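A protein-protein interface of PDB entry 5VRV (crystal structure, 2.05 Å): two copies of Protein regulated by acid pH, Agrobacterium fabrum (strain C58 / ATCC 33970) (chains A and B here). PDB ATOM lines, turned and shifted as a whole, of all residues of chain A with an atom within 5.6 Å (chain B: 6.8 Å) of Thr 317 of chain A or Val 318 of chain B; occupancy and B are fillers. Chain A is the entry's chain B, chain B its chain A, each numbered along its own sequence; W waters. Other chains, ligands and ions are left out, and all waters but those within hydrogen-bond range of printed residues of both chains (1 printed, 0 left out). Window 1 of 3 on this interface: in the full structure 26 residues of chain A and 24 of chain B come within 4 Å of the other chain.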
ATOM      1  N   HIS A 275     -28.275 -12.348 -11.793  1.00  0.00           N
ATOM      2  CA  HIS A 275     -29.081 -11.141 -11.991  1.00  0.00           C
ATOM      3  C   HIS A 275     -30.551 -11.454 -11.665  1.00  0.00           C
ATOM      4  O   HIS A 275     -31.184 -10.711 -10.922  1.00  0.00           O
ATOM      5  CB  HIS A 275     -28.961 -10.609 -13.419  1.00  0.00           C
ATOM      6  CG  HIS A 275     -29.894  -9.481 -13.706  1.00  0.00           C
ATOM      7  ND1 HIS A 275     -29.586  -8.167 -13.420  1.00  0.00           N
ATOM      8  CD2 HIS A 275     -31.142  -9.474 -14.229  1.00  0.00           C
ATOM      9  CE1 HIS A 275     -30.605  -7.401 -13.760  1.00  0.00           C
ATOM     10  NE2 HIS A 275     -31.567  -8.170 -14.240  1.00  0.00           N
ATOM     11  N   ARG A 278     -31.277 -11.908  -7.995  1.00  0.00           N
ATOM     12  CA  ARG A 278     -31.132 -10.618  -7.343  1.00  0.00           C
ATOM     13  C   ARG A 278     -32.351  -9.698  -7.485  1.00  0.00           C
ATOM     14  O   ARG A 278     -32.692  -8.996  -6.534  1.00  0.00           O
ATOM     15  CB  ARG A 278     -29.849  -9.925  -7.829  1.00  0.00           C
ATOM     16  CG  ARG A 278     -29.734  -8.477  -7.412  1.00  0.00           C
ATOM     17  CD  ARG A 278     -28.324  -7.916  -7.568  1.00  0.00           C
ATOM     18  NE  ARG A 278     -27.721  -8.168  -8.874  1.00  0.00           N
ATOM     19  CZ  ARG A 278     -26.773  -9.074  -9.092  1.00  0.00           C
ATOM     20  NH1 ARG A 278     -26.297  -9.790  -8.084  1.00  0.00           N
ATOM     21  NH2 ARG A 278     -26.280  -9.246 -10.312  1.00  0.00           N
ATOM     22  N   PHE A 279     -33.029  -9.725  -8.634  1.00  0.00           N
ATOM     23  CA  PHE A 279     -34.182  -8.833  -8.846  1.00  0.00           C
ATOM     24  C   PHE A 279     -35.560  -9.397  -9.209  1.00  0.00           C
ATOM     25  O   PHE A 279     -36.521  -8.650  -9.167  1.00  0.00           O
ATOM     26  CB  PHE A 279     -33.847  -7.806  -9.950  1.00  0.00           C
ATOM     27  CG  PHE A 279     -32.684  -6.906  -9.629  1.00  0.00           C
ATOM     28  CD1 PHE A 279     -32.772  -5.974  -8.596  1.00  0.00           C
ATOM     29  CD2 PHE A 279     -31.529  -6.933 -10.411  1.00  0.00           C
ATOM     30  CE1 PHE A 279     -31.707  -5.128  -8.316  1.00  0.00           C
ATOM     31  CE2 PHE A 279     -30.466  -6.085 -10.139  1.00  0.00           C
ATOM     32  CZ  PHE A 279     -30.558  -5.180  -9.087  1.00  0.00           C
ATOM     33  N   ALA A 312     -22.981  -3.633 -19.224  1.00  0.00           N
ATOM     34  CA  ALA A 312     -24.236  -2.903 -19.240  1.00  0.00           C
ATOM     35  C   ALA A 312     -25.121  -3.324 -18.078  1.00  0.00           C
ATOM     36  O   ALA A 312     -25.732  -2.476 -17.424  1.00  0.00           O
ATOM     37  CB  ALA A 312     -24.970  -3.113 -20.547  1.00  0.00           C
ATOM     38  N   LEU A 313     -25.161  -4.630 -17.814  1.00  0.00           N
ATOM     39  CA  LEU A 313     -25.986  -5.168 -16.750  1.00  0.00           C
ATOM     40  C   LEU A 313     -25.493  -4.684 -15.375  1.00  0.00           C
ATOM     41  O   LEU A 313     -26.292  -4.525 -14.454  1.00  0.00           O
ATOM     42  CB  LEU A 313     -26.025  -6.688 -16.853  1.00  0.00           C
ATOM     43  CG  LEU A 313     -27.138  -7.442 -16.159  1.00  0.00           C
ATOM     44  CD1 LEU A 313     -28.505  -6.951 -16.611  1.00  0.00           C
ATOM     45  CD2 LEU A 313     -26.972  -8.917 -16.486  1.00  0.00           C
ATOM     46  N   MET A 314     -24.191  -4.432 -15.248  1.00  0.00           N
ATOM     47  CA  MET A 314     -23.646  -3.900 -14.007  1.00  0.00           C
ATOM     48  C   MET A 314     -24.132  -2.477 -13.844  1.00  0.00           C
ATOM     49  O   MET A 314     -24.500  -2.078 -12.734  1.00  0.00           O
ATOM     50  CB  MET A 314     -22.126  -3.943 -13.938  1.00  0.00           C
ATOM     51  CG  MET A 314     -21.635  -3.528 -12.542  1.00  0.00           C
ATOM     52  SD  MET A 314     -20.614  -4.975 -11.667  1.00  0.00           S
ATOM     53  CE  MET A 314     -19.221  -5.087 -13.046  1.00  0.00           C
ATOM     54  N   ASP A 315     -24.128  -1.696 -14.926  1.00  0.00           N
ATOM     55  CA  ASP A 315     -24.640  -0.308 -14.846  1.00  0.00           C
ATOM     56  C   ASP A 315     -26.146  -0.296 -14.504  1.00  0.00           C
ATOM     57  O   ASP A 315     -26.592   0.528 -13.707  1.00  0.00           O
ATOM     58  CB  ASP A 315     -24.323   0.495 -16.119  1.00  0.00           C
ATOM     59  CG  ASP A 315     -22.844   0.901 -16.200  1.00  0.00           C
ATOM     60  OD1 ASP A 315     -22.272   1.275 -15.159  1.00  0.00           O
ATOM     61  OD2 ASP A 315     -22.276   0.903 -17.298  1.00  0.00           O
ATOM     62  N   ALA A 316     -26.894  -1.239 -15.081  1.00  0.00           N
ATOM     63  CA  ALA A 316     -28.325  -1.401 -14.794  1.00  0.00           C
ATOM     64  C   ALA A 316     -28.548  -1.727 -13.319  1.00  0.00           C
ATOM     65  O   ALA A 316     -29.476  -1.211 -12.700  1.00  0.00           O
ATOM     66  CB  ALA A 316     -28.932  -2.509 -15.657  1.00  0.00           C
ATOM     67  N   THR A 317     -27.679  -2.571 -12.776  1.00  0.00           N
ATOM     68  CA  THR A 317     -27.739  -3.005 -11.369  1.00  0.00           C
ATOM     69  C   THR A 317     -27.552  -1.826 -10.410  1.00  0.00           C
ATOM     70  O   THR A 317     -28.173  -1.798  -9.358  1.00  0.00           O
ATOM     71  CB  THR A 317     -26.707  -4.131 -11.099  1.00  0.00           C
ATOM     72  OG1 THR A 317     -27.030  -5.260 -11.922  1.00  0.00           O
ATOM     73  CG2 THR A 317     -26.678  -4.555  -9.632  1.00  0.00           C
ATOM     74  N   VAL A 318     -26.702  -0.868 -10.780  1.00  0.00           N
ATOM     75  CA  VAL A 318     -26.471   0.348  -9.974  1.00  0.00           C
ATOM     76  C   VAL A 318     -27.686   1.262 -10.061  1.00  0.00           C
ATOM     77  O   VAL A 318     -28.095   1.875  -9.092  1.00  0.00           O
ATOM     78  CB  VAL A 318     -25.241   1.133 -10.491  1.00  0.00           C
ATOM     79  CG1 VAL A 318     -25.099   2.492  -9.803  1.00  0.00           C
ATOM     80  CG2 VAL A 318     -23.978   0.309 -10.314  1.00  0.00           C
ATOM     81  N   LEU A 319     -28.227   1.354 -11.266  1.00  0.00           N
ATOM     82  CA  LEU A 319     -29.390   2.171 -11.574  1.00  0.00           C
ATOM     83  C   LEU A 319     -30.631   1.750 -10.755  1.00  0.00           C
ATOM     84  O   LEU A 319     -31.419   2.598 -10.289  1.00  0.00           O
ATOM     85  CB  LEU A 319     -29.627   2.010 -13.074  1.00  0.00           C
ATOM     86  CG  LEU A 319     -30.063   3.143 -13.976  1.00  0.00           C
ATOM     87  CD1 LEU A 319     -29.318   4.434 -13.668  1.00  0.00           C
ATOM     88  CD2 LEU A 319     -29.804   2.674 -15.413  1.00  0.00           C
ATOM     89  N   ILE A 320     -30.786   0.445 -10.568  1.00  0.00           N
ATOM     90  CA  ILE A 320     -31.898  -0.124  -9.803  1.00  0.00           C
ATOM     91  C   ILE A 320     -31.609  -0.141  -8.291  1.00  0.00           C
ATOM     92  O   ILE A 320     -32.457   0.246  -7.490  1.00  0.00           O
ATOM     93  CB  ILE A 320     -32.207  -1.558 -10.279  1.00  0.00           C
ATOM     94  CG1 ILE A 320     -32.574  -1.569 -11.763  1.00  0.00           C
ATOM     95  CG2 ILE A 320     -33.343  -2.168  -9.469  1.00  0.00           C
ATOM     96  CD1 ILE A 320     -32.442  -2.931 -12.413  1.00  0.00           C
ATOM     97  N   SER A 321     -30.408  -0.547  -7.905  1.00  0.00           N
ATOM     98  CA  SER A 321     -30.031  -0.647  -6.478  1.00  0.00           C
ATOM     99  C   SER A 321     -29.820   0.687  -5.766  1.00  0.00           C
ATOM    100  O   SER A 321     -30.288   0.859  -4.635  1.00  0.00           O
ATOM    101  CB  SER A 321     -28.766  -1.486  -6.329  1.00  0.00           C
ATOM    102  OG  SER A 321     -28.929  -2.716  -6.978  1.00  0.00           O
ATOM    103  N   GLY A 322     -29.092   1.605  -6.412  1.00  0.00           N
ATOM    104  CA  GLY A 322     -28.813   2.939  -5.864  1.00  0.00           C
ATOM    105  C   GLY A 322     -29.538   3.898  -6.772  1.00  0.00           C
ATOM    106  O   GLY A 322     -30.737   4.133  -6.611  1.00  0.00           O
ATOM    107  N   GLN B  46     -24.370 -10.606   0.209  1.00  0.00           N
ATOM    108  CA  GLN B  46     -25.220 -10.175  -0.900  1.00  0.00           C
ATOM    109  C   GLN B  46     -25.285 -11.256  -1.975  1.00  0.00           C
ATOM    110  O   GLN B  46     -24.265 -11.616  -2.569  1.00  0.00           O
ATOM    111  CB  GLN B  46     -24.686  -8.866  -1.477  1.00  0.00           C
ATOM    112  CG  GLN B  46     -25.435  -8.346  -2.689  1.00  0.00           C
ATOM    113  CD  GLN B  46     -26.912  -8.136  -2.431  1.00  0.00           C
ATOM    114  OE1 GLN B  46     -27.297  -7.492  -1.448  1.00  0.00           O
ATOM    115  NE2 GLN B  46     -27.748  -8.645  -3.330  1.00  0.00           N
ATOM    116  N   ARG B 171     -23.463   2.686   1.012  1.00  0.00           N
ATOM    117  CA  ARG B 171     -23.241   1.823   2.160  1.00  0.00           C
ATOM    118  C   ARG B 171     -21.912   1.054   1.992  1.00  0.00           C
ATOM    119  O   ARG B 171     -21.205   1.219   0.989  1.00  0.00           O
ATOM    120  CB  ARG B 171     -24.357   0.777   2.242  1.00  0.00           C
ATOM    121  CG  ARG B 171     -25.740   1.258   2.621  1.00  0.00           C
ATOM    122  CD  ARG B 171     -25.810   1.722   4.053  1.00  0.00           C
ATOM    123  NE  ARG B 171     -27.181   2.057   4.434  1.00  0.00           N
ATOM    124  CZ  ARG B 171     -27.782   3.239   4.260  1.00  0.00           C
ATOM    125  NH1 ARG B 171     -27.164   4.256   3.668  1.00  0.00           N
ATOM    126  NH2 ARG B 171     -29.037   3.395   4.673  1.00  0.00           N
ATOM    127  N   PHE B 279     -16.883   4.228  -8.466  1.00  0.00           N
ATOM    128  CA  PHE B 279     -16.796   4.498  -7.027  1.00  0.00           C
ATOM    129  C   PHE B 279     -15.595   5.268  -6.496  1.00  0.00           C
ATOM    130  O   PHE B 279     -15.630   5.683  -5.345  1.00  0.00           O
ATOM    131  CB  PHE B 279     -16.817   3.160  -6.245  1.00  0.00           C
ATOM    132  CG  PHE B 279     -18.090   2.377  -6.387  1.00  0.00           C
ATOM    133  CD1 PHE B 279     -19.284   2.872  -5.862  1.00  0.00           C
ATOM    134  CD2 PHE B 279     -18.093   1.125  -6.999  1.00  0.00           C
ATOM    135  CE1 PHE B 279     -20.453   2.155  -5.974  1.00  0.00           C
ATOM    136  CE2 PHE B 279     -19.258   0.405  -7.107  1.00  0.00           C
ATOM    137  CZ  PHE B 279     -20.439   0.921  -6.594  1.00  0.00           C
ATOM    138  N   LEU B 313     -17.585  -8.849  -7.634  1.00  0.00           N
ATOM    139  CA  LEU B 313     -17.558  -7.402  -7.764  1.00  0.00           C
ATOM    140  C   LEU B 313     -18.981  -6.870  -8.007  1.00  0.00           C
ATOM    141  O   LEU B 313     -19.336  -5.789  -7.530  1.00  0.00           O
ATOM    142  CB  LEU B 313     -16.584  -6.998  -8.871  1.00  0.00           C
ATOM    143  CG  LEU B 313     -16.016  -5.587  -8.831  1.00  0.00           C
ATOM    144  CD1 LEU B 313     -15.413  -5.273  -7.469  1.00  0.00           C
ATOM    145  CD2 LEU B 313     -14.964  -5.468  -9.917  1.00  0.00           C
ATOM    146  N   MET B 314     -19.807  -7.661  -8.690  1.00  0.00           N
ATOM    147  CA  MET B 314     -21.206  -7.289  -8.927  1.00  0.00           C
ATOM    148  C   MET B 314     -21.978  -7.276  -7.618  1.00  0.00           C
ATOM    149  O   MET B 314     -22.773  -6.356  -7.376  1.00  0.00           O
ATOM    150  CB  MET B 314     -21.812  -8.221  -9.968  1.00  0.00           C
ATOM    151  CG  MET B 314     -23.298  -8.044 -10.168  1.00  0.00           C
ATOM    152  SD  MET B 314     -23.635  -6.615 -11.484  1.00  0.00           S
ATOM    153  CE  MET B 314     -23.639  -7.776 -13.067  1.00  0.00           C
ATOM    154  N   ASP B 315     -21.754  -8.271  -6.759  1.00  0.00           N
ATOM    155  CA  ASP B 315     -22.418  -8.305  -5.449  1.00  0.00           C
ATOM    156  C   ASP B 315     -21.922  -7.131  -4.607  1.00  0.00           C
ATOM    157  O   ASP B 315     -22.712  -6.493  -3.910  1.00  0.00           O
ATOM    158  CB  ASP B 315     -22.199  -9.642  -4.731  1.00  0.00           C
ATOM    159  CG  ASP B 315     -22.955 -10.798  -5.388  1.00  0.00           C
ATOM    160  OD1 ASP B 315     -24.128 -10.640  -5.743  1.00  0.00           O
ATOM    161  OD2 ASP B 315     -22.390 -11.889  -5.493  1.00  0.00           O
ATOM    162  N   ALA B 316     -20.617  -6.839  -4.690  1.00  0.00           N
ATOM    163  CA  ALA B 316     -20.040  -5.697  -3.982  1.00  0.00           C
ATOM    164  C   ALA B 316     -20.667  -4.395  -4.476  1.00  0.00           C
ATOM    165  O   ALA B 316     -20.888  -3.497  -3.700  1.00  0.00           O
ATOM    166  CB  ALA B 316     -18.526  -5.647  -4.150  1.00  0.00           C
ATOM    167  N   THR B 317     -20.985  -4.328  -5.763  1.00  0.00           N
ATOM    168  CA  THR B 317     -21.592  -3.143  -6.353  1.00  0.00           C
ATOM    169  C   THR B 317     -22.968  -2.869  -5.745  1.00  0.00           C
ATOM    170  O   THR B 317     -23.322  -1.705  -5.504  1.00  0.00           O
ATOM    171  CB  THR B 317     -21.685  -3.268  -7.882  1.00  0.00           C
ATOM    172  OG1 THR B 317     -20.366  -3.425  -8.415  1.00  0.00           O
ATOM    173  CG2 THR B 317     -22.335  -2.034  -8.501  1.00  0.00           C
ATOM    174  N   VAL B 318     -23.717  -3.939  -5.471  1.00  0.00           N
ATOM    175  CA  VAL B 318     -25.042  -3.841  -4.846  1.00  0.00           C
ATOM    176  C   VAL B 318     -24.888  -3.428  -3.375  1.00  0.00           C
ATOM    177  O   VAL B 318     -25.634  -2.572  -2.888  1.00  0.00           O
ATOM    178  CB  VAL B 318     -25.816  -5.179  -4.938  1.00  0.00           C
ATOM    179  CG1 VAL B 318     -27.097  -5.161  -4.104  1.00  0.00           C
ATOM    180  CG2 VAL B 318     -26.119  -5.512  -6.378  1.00  0.00           C
ATOM    181  N   LEU B 319     -23.928  -4.037  -2.677  1.00  0.00           N
ATOM    182  CA  LEU B 319     -23.675  -3.710  -1.260  1.00  0.00           C
ATOM    183  C   LEU B 319     -23.388  -2.230  -1.041  1.00  0.00           C
ATOM    184  O   LEU B 319     -23.800  -1.645  -0.034  1.00  0.00           O
ATOM    185  CB  LEU B 319     -22.493  -4.525  -0.696  1.00  0.00           C
ATOM    186  CG  LEU B 319     -22.707  -5.992  -0.343  1.00  0.00           C
ATOM    187  CD1 LEU B 319     -21.398  -6.667   0.046  1.00  0.00           C
ATOM    188  CD2 LEU B 319     -23.710  -6.109   0.797  1.00  0.00           C
ATOM    189  N   ILE B 320     -22.673  -1.641  -1.989  1.00  0.00           N
ATOM    190  CA  ILE B 320     -22.300  -0.244  -1.909  1.00  0.00           C
ATOM    191  C   ILE B 320     -23.410   0.673  -2.394  1.00  0.00           C
ATOM    192  O   ILE B 320     -23.736   1.659  -1.732  1.00  0.00           O
ATOM    193  CB  ILE B 320     -21.017   0.042  -2.724  1.00  0.00           C
ATOM    194  CG1 ILE B 320     -19.841  -0.778  -2.176  1.00  0.00           C
ATOM    195  CG2 ILE B 320     -20.672   1.526  -2.648  1.00  0.00           C
ATOM    196  CD1 ILE B 320     -18.669  -0.895  -3.146  1.00  0.00           C
ATOM    197  N   SER B 321     -23.978   0.346  -3.550  1.00  0.00           N
ATOM    198  CA  SER B 321     -24.998   1.187  -4.184  1.00  0.00           C
ATOM    199  C   SER B 321     -26.345   1.201  -3.484  1.00  0.00           C
ATOM    200  O   SER B 321     -26.960   2.259  -3.339  1.00  0.00           O
ATOM    201  CB  SER B 321     -25.198   0.761  -5.645  1.00  0.00           C
ATOM    202  OG  SER B 321     -23.985   0.884  -6.364  1.00  0.00           O
ATOM    203  N   GLY B 322     -26.810   0.032  -3.086  1.00  0.00           N
ATOM    204  CA  GLY B 322     -28.097  -0.102  -2.410  1.00  0.00           C
ATOM    205  C   GLY B 322     -27.762  -0.649  -1.048  1.00  0.00           C
ATOM    206  O   GLY B 322     -27.431   0.096  -0.143  1.00  0.00           O
ATOM    207  N   GLY B 323     -27.834  -1.964  -0.923  1.00  0.00           N
ATOM    208  CA  GLY B 323     -27.454  -2.616   0.310  1.00  0.00           C
ATOM    209  C   GLY B 323     -28.432  -2.567   1.457  1.00  0.00           C
ATOM    210  O   GLY B 323     -29.637  -2.375   1.274  1.00  0.00           O
ATOM    211  N   VAL B 324     -27.886  -2.724   2.650  1.00  0.00           N
ATOM    212  CA  VAL B 324     -28.694  -2.809   3.858  1.00  0.00           C
ATOM    213  C   VAL B 324     -29.157  -1.465   4.385  1.00  0.00           C
ATOM    214  O   VAL B 324     -28.528  -0.438   4.141  1.00  0.00           O
ATOM    215  CB  VAL B 324     -27.959  -3.578   4.997  1.00  0.00           C
ATOM    216  CG1 VAL B 324     -27.560  -4.981   4.541  1.00  0.00           C
ATOM    217  CG2 VAL B 324     -26.740  -2.828   5.495  1.00  0.00           C
HETATM  218  O   HOH W   1     -26.668  -9.701  -5.580  1.00  0.00           O
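Met 314 of chain A touches its own counterpart, Met 314 of chain B. Met 314 of chain A touches Thr 317 of chain B, and with the chains exchanged Thr 317 of chain A touches Met 314 of chain B. Thr 317 of chain A touches Val 318 of chain B, and with the chains exchanged Val 318 of chain A touches Thr 317 of chain B. Val 318 of chain A touches Ser 321 of chain B, but with the chains exchanged Ser 321 of chain A does not touch Val 318 of chain B (4.01 Å). Positions printed for both chains: 279, 313, 314, 315, 316, 317, 318, 319, 320, 321 and 322. Of the 12 pairs that touch across the chains among the printed residues, 8 have their exchanged pair printed and touching as well.
Printed residues of chain B that touch a printed residue of chain A: Met 314, Asp 315, Thr 317, Val 318, Ser 321 and Gly 322. Hydrophobic or aromatic side chains of chain B that line the printed part of chain A: Met 314 and Val 318. Along chain B the printed residues that touch a printed residue of chain A span positions 314 to 322. Among the printed residues, Asp or Glu carboxylates within 4 Å of a Lys or Arg side-chain nitrogen of the other chain: Arg 278 of chain A with Asp 315 of chain B.
OG1 of Thr 317 of chain A lies within hydrogen-bond range of O of Leu 313 of chain A (2.7 Å). The side-chain hydroxyl of Thr 317 of chain B sits at hydrogen-bond distance from the backbone carbonyl oxygen of Leu 313 of chain B. The backbone carbonyl oxygen of Thr 317 of chain A sits at hydrogen-bond distance from the side-chain hydroxyl of Ser 321 of chain A (2.7 Å). The backbone carbonyl oxygen of Val 318 of chain B is in hydrogen-bond range of the backbone NH of Gly 323 of chain B. The backbone carbonyl oxygen (O) of Thr 317 of chain B sits at hydrogen-bond distance from the side-chain hydroxyl (OG) of Ser 321 of chain B (2.8 Å).
Of chain B, only Met 314 and Val 318 come within 4 Å of Thr 317 of chain A. Printed residues of chain A within 4 Å of Val 318 of chain B: Arg 278 (3.5 Å) and Thr 317 (3.4 Å). Of the printed residues of chain A, Ser 321 of chain B touches Val 318 (3.96 Å), Ser 321 (3.8 Å) and Gly 322 (3.2 Å). Printed residues of chain B within 4 Å of Val 318 of chain A: Thr 317 and Ser 321. Ile 320 of chain B touches none of the printed residues of chain A. Ala 312 of chain A touches none of the printed residues of chain B. The nearest residue of chain B that does not touch Thr 317 of chain A is Thr 317 of chain B (5.1 Å).
CG of Met 314 of chain B touches NH2 of Arg 278 of chain A, at 3.2 Å. CG2 of Val 318 of chain B touches CD of Arg 278 of chain A, at 3.5 Å. Thr 317 of chain A touches Val 318 of chain B. Val 318 of chain A touches Thr 317 of chain B (CG2 to CG2, 3.4 Å). Val 318 of chain A touches Ser 321 of chain B (CG1 to OG, 3.96 Å). O of Ser 321 of chain B touches O of Ser 321 of chain A, 3.8 Å away. O of Ser 321 of chain A touches CA of Gly 322 of chain B, 3.3 Å away. Ser 321 of chain B touches Gly 322 of chain A.
Water W1 lies within hydrogen-bond range of the guanidinium group of Arg 278 of chain A (2.5 Å), the side-chain amide nitrogen of Gln 46 of chain B (2.7 Å) and the side-chain carboxylate of Asp 315 of chain B (2.7 Å).
The side-chain hydroxyl (OG1) of Thr 317 of chain B is in hydrogen-bond range of the side-chain sulfur (SD) of Met 314 of chain A (3.6 Å). OD1 of Asp 315 of chain B is in salt-bridge range of NH1 of Arg 278 of chain A, at 3.3 Å. The side-chain sulfur (SD) of Met 314 of chain B is in hydrogen-bond range of the side-chain hydroxyl (OG1) of Thr 317 of chain A (3.7 Å). SD of Met 314 of chain B lies close to SD of Met 314 of chain A (3.4 Å).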
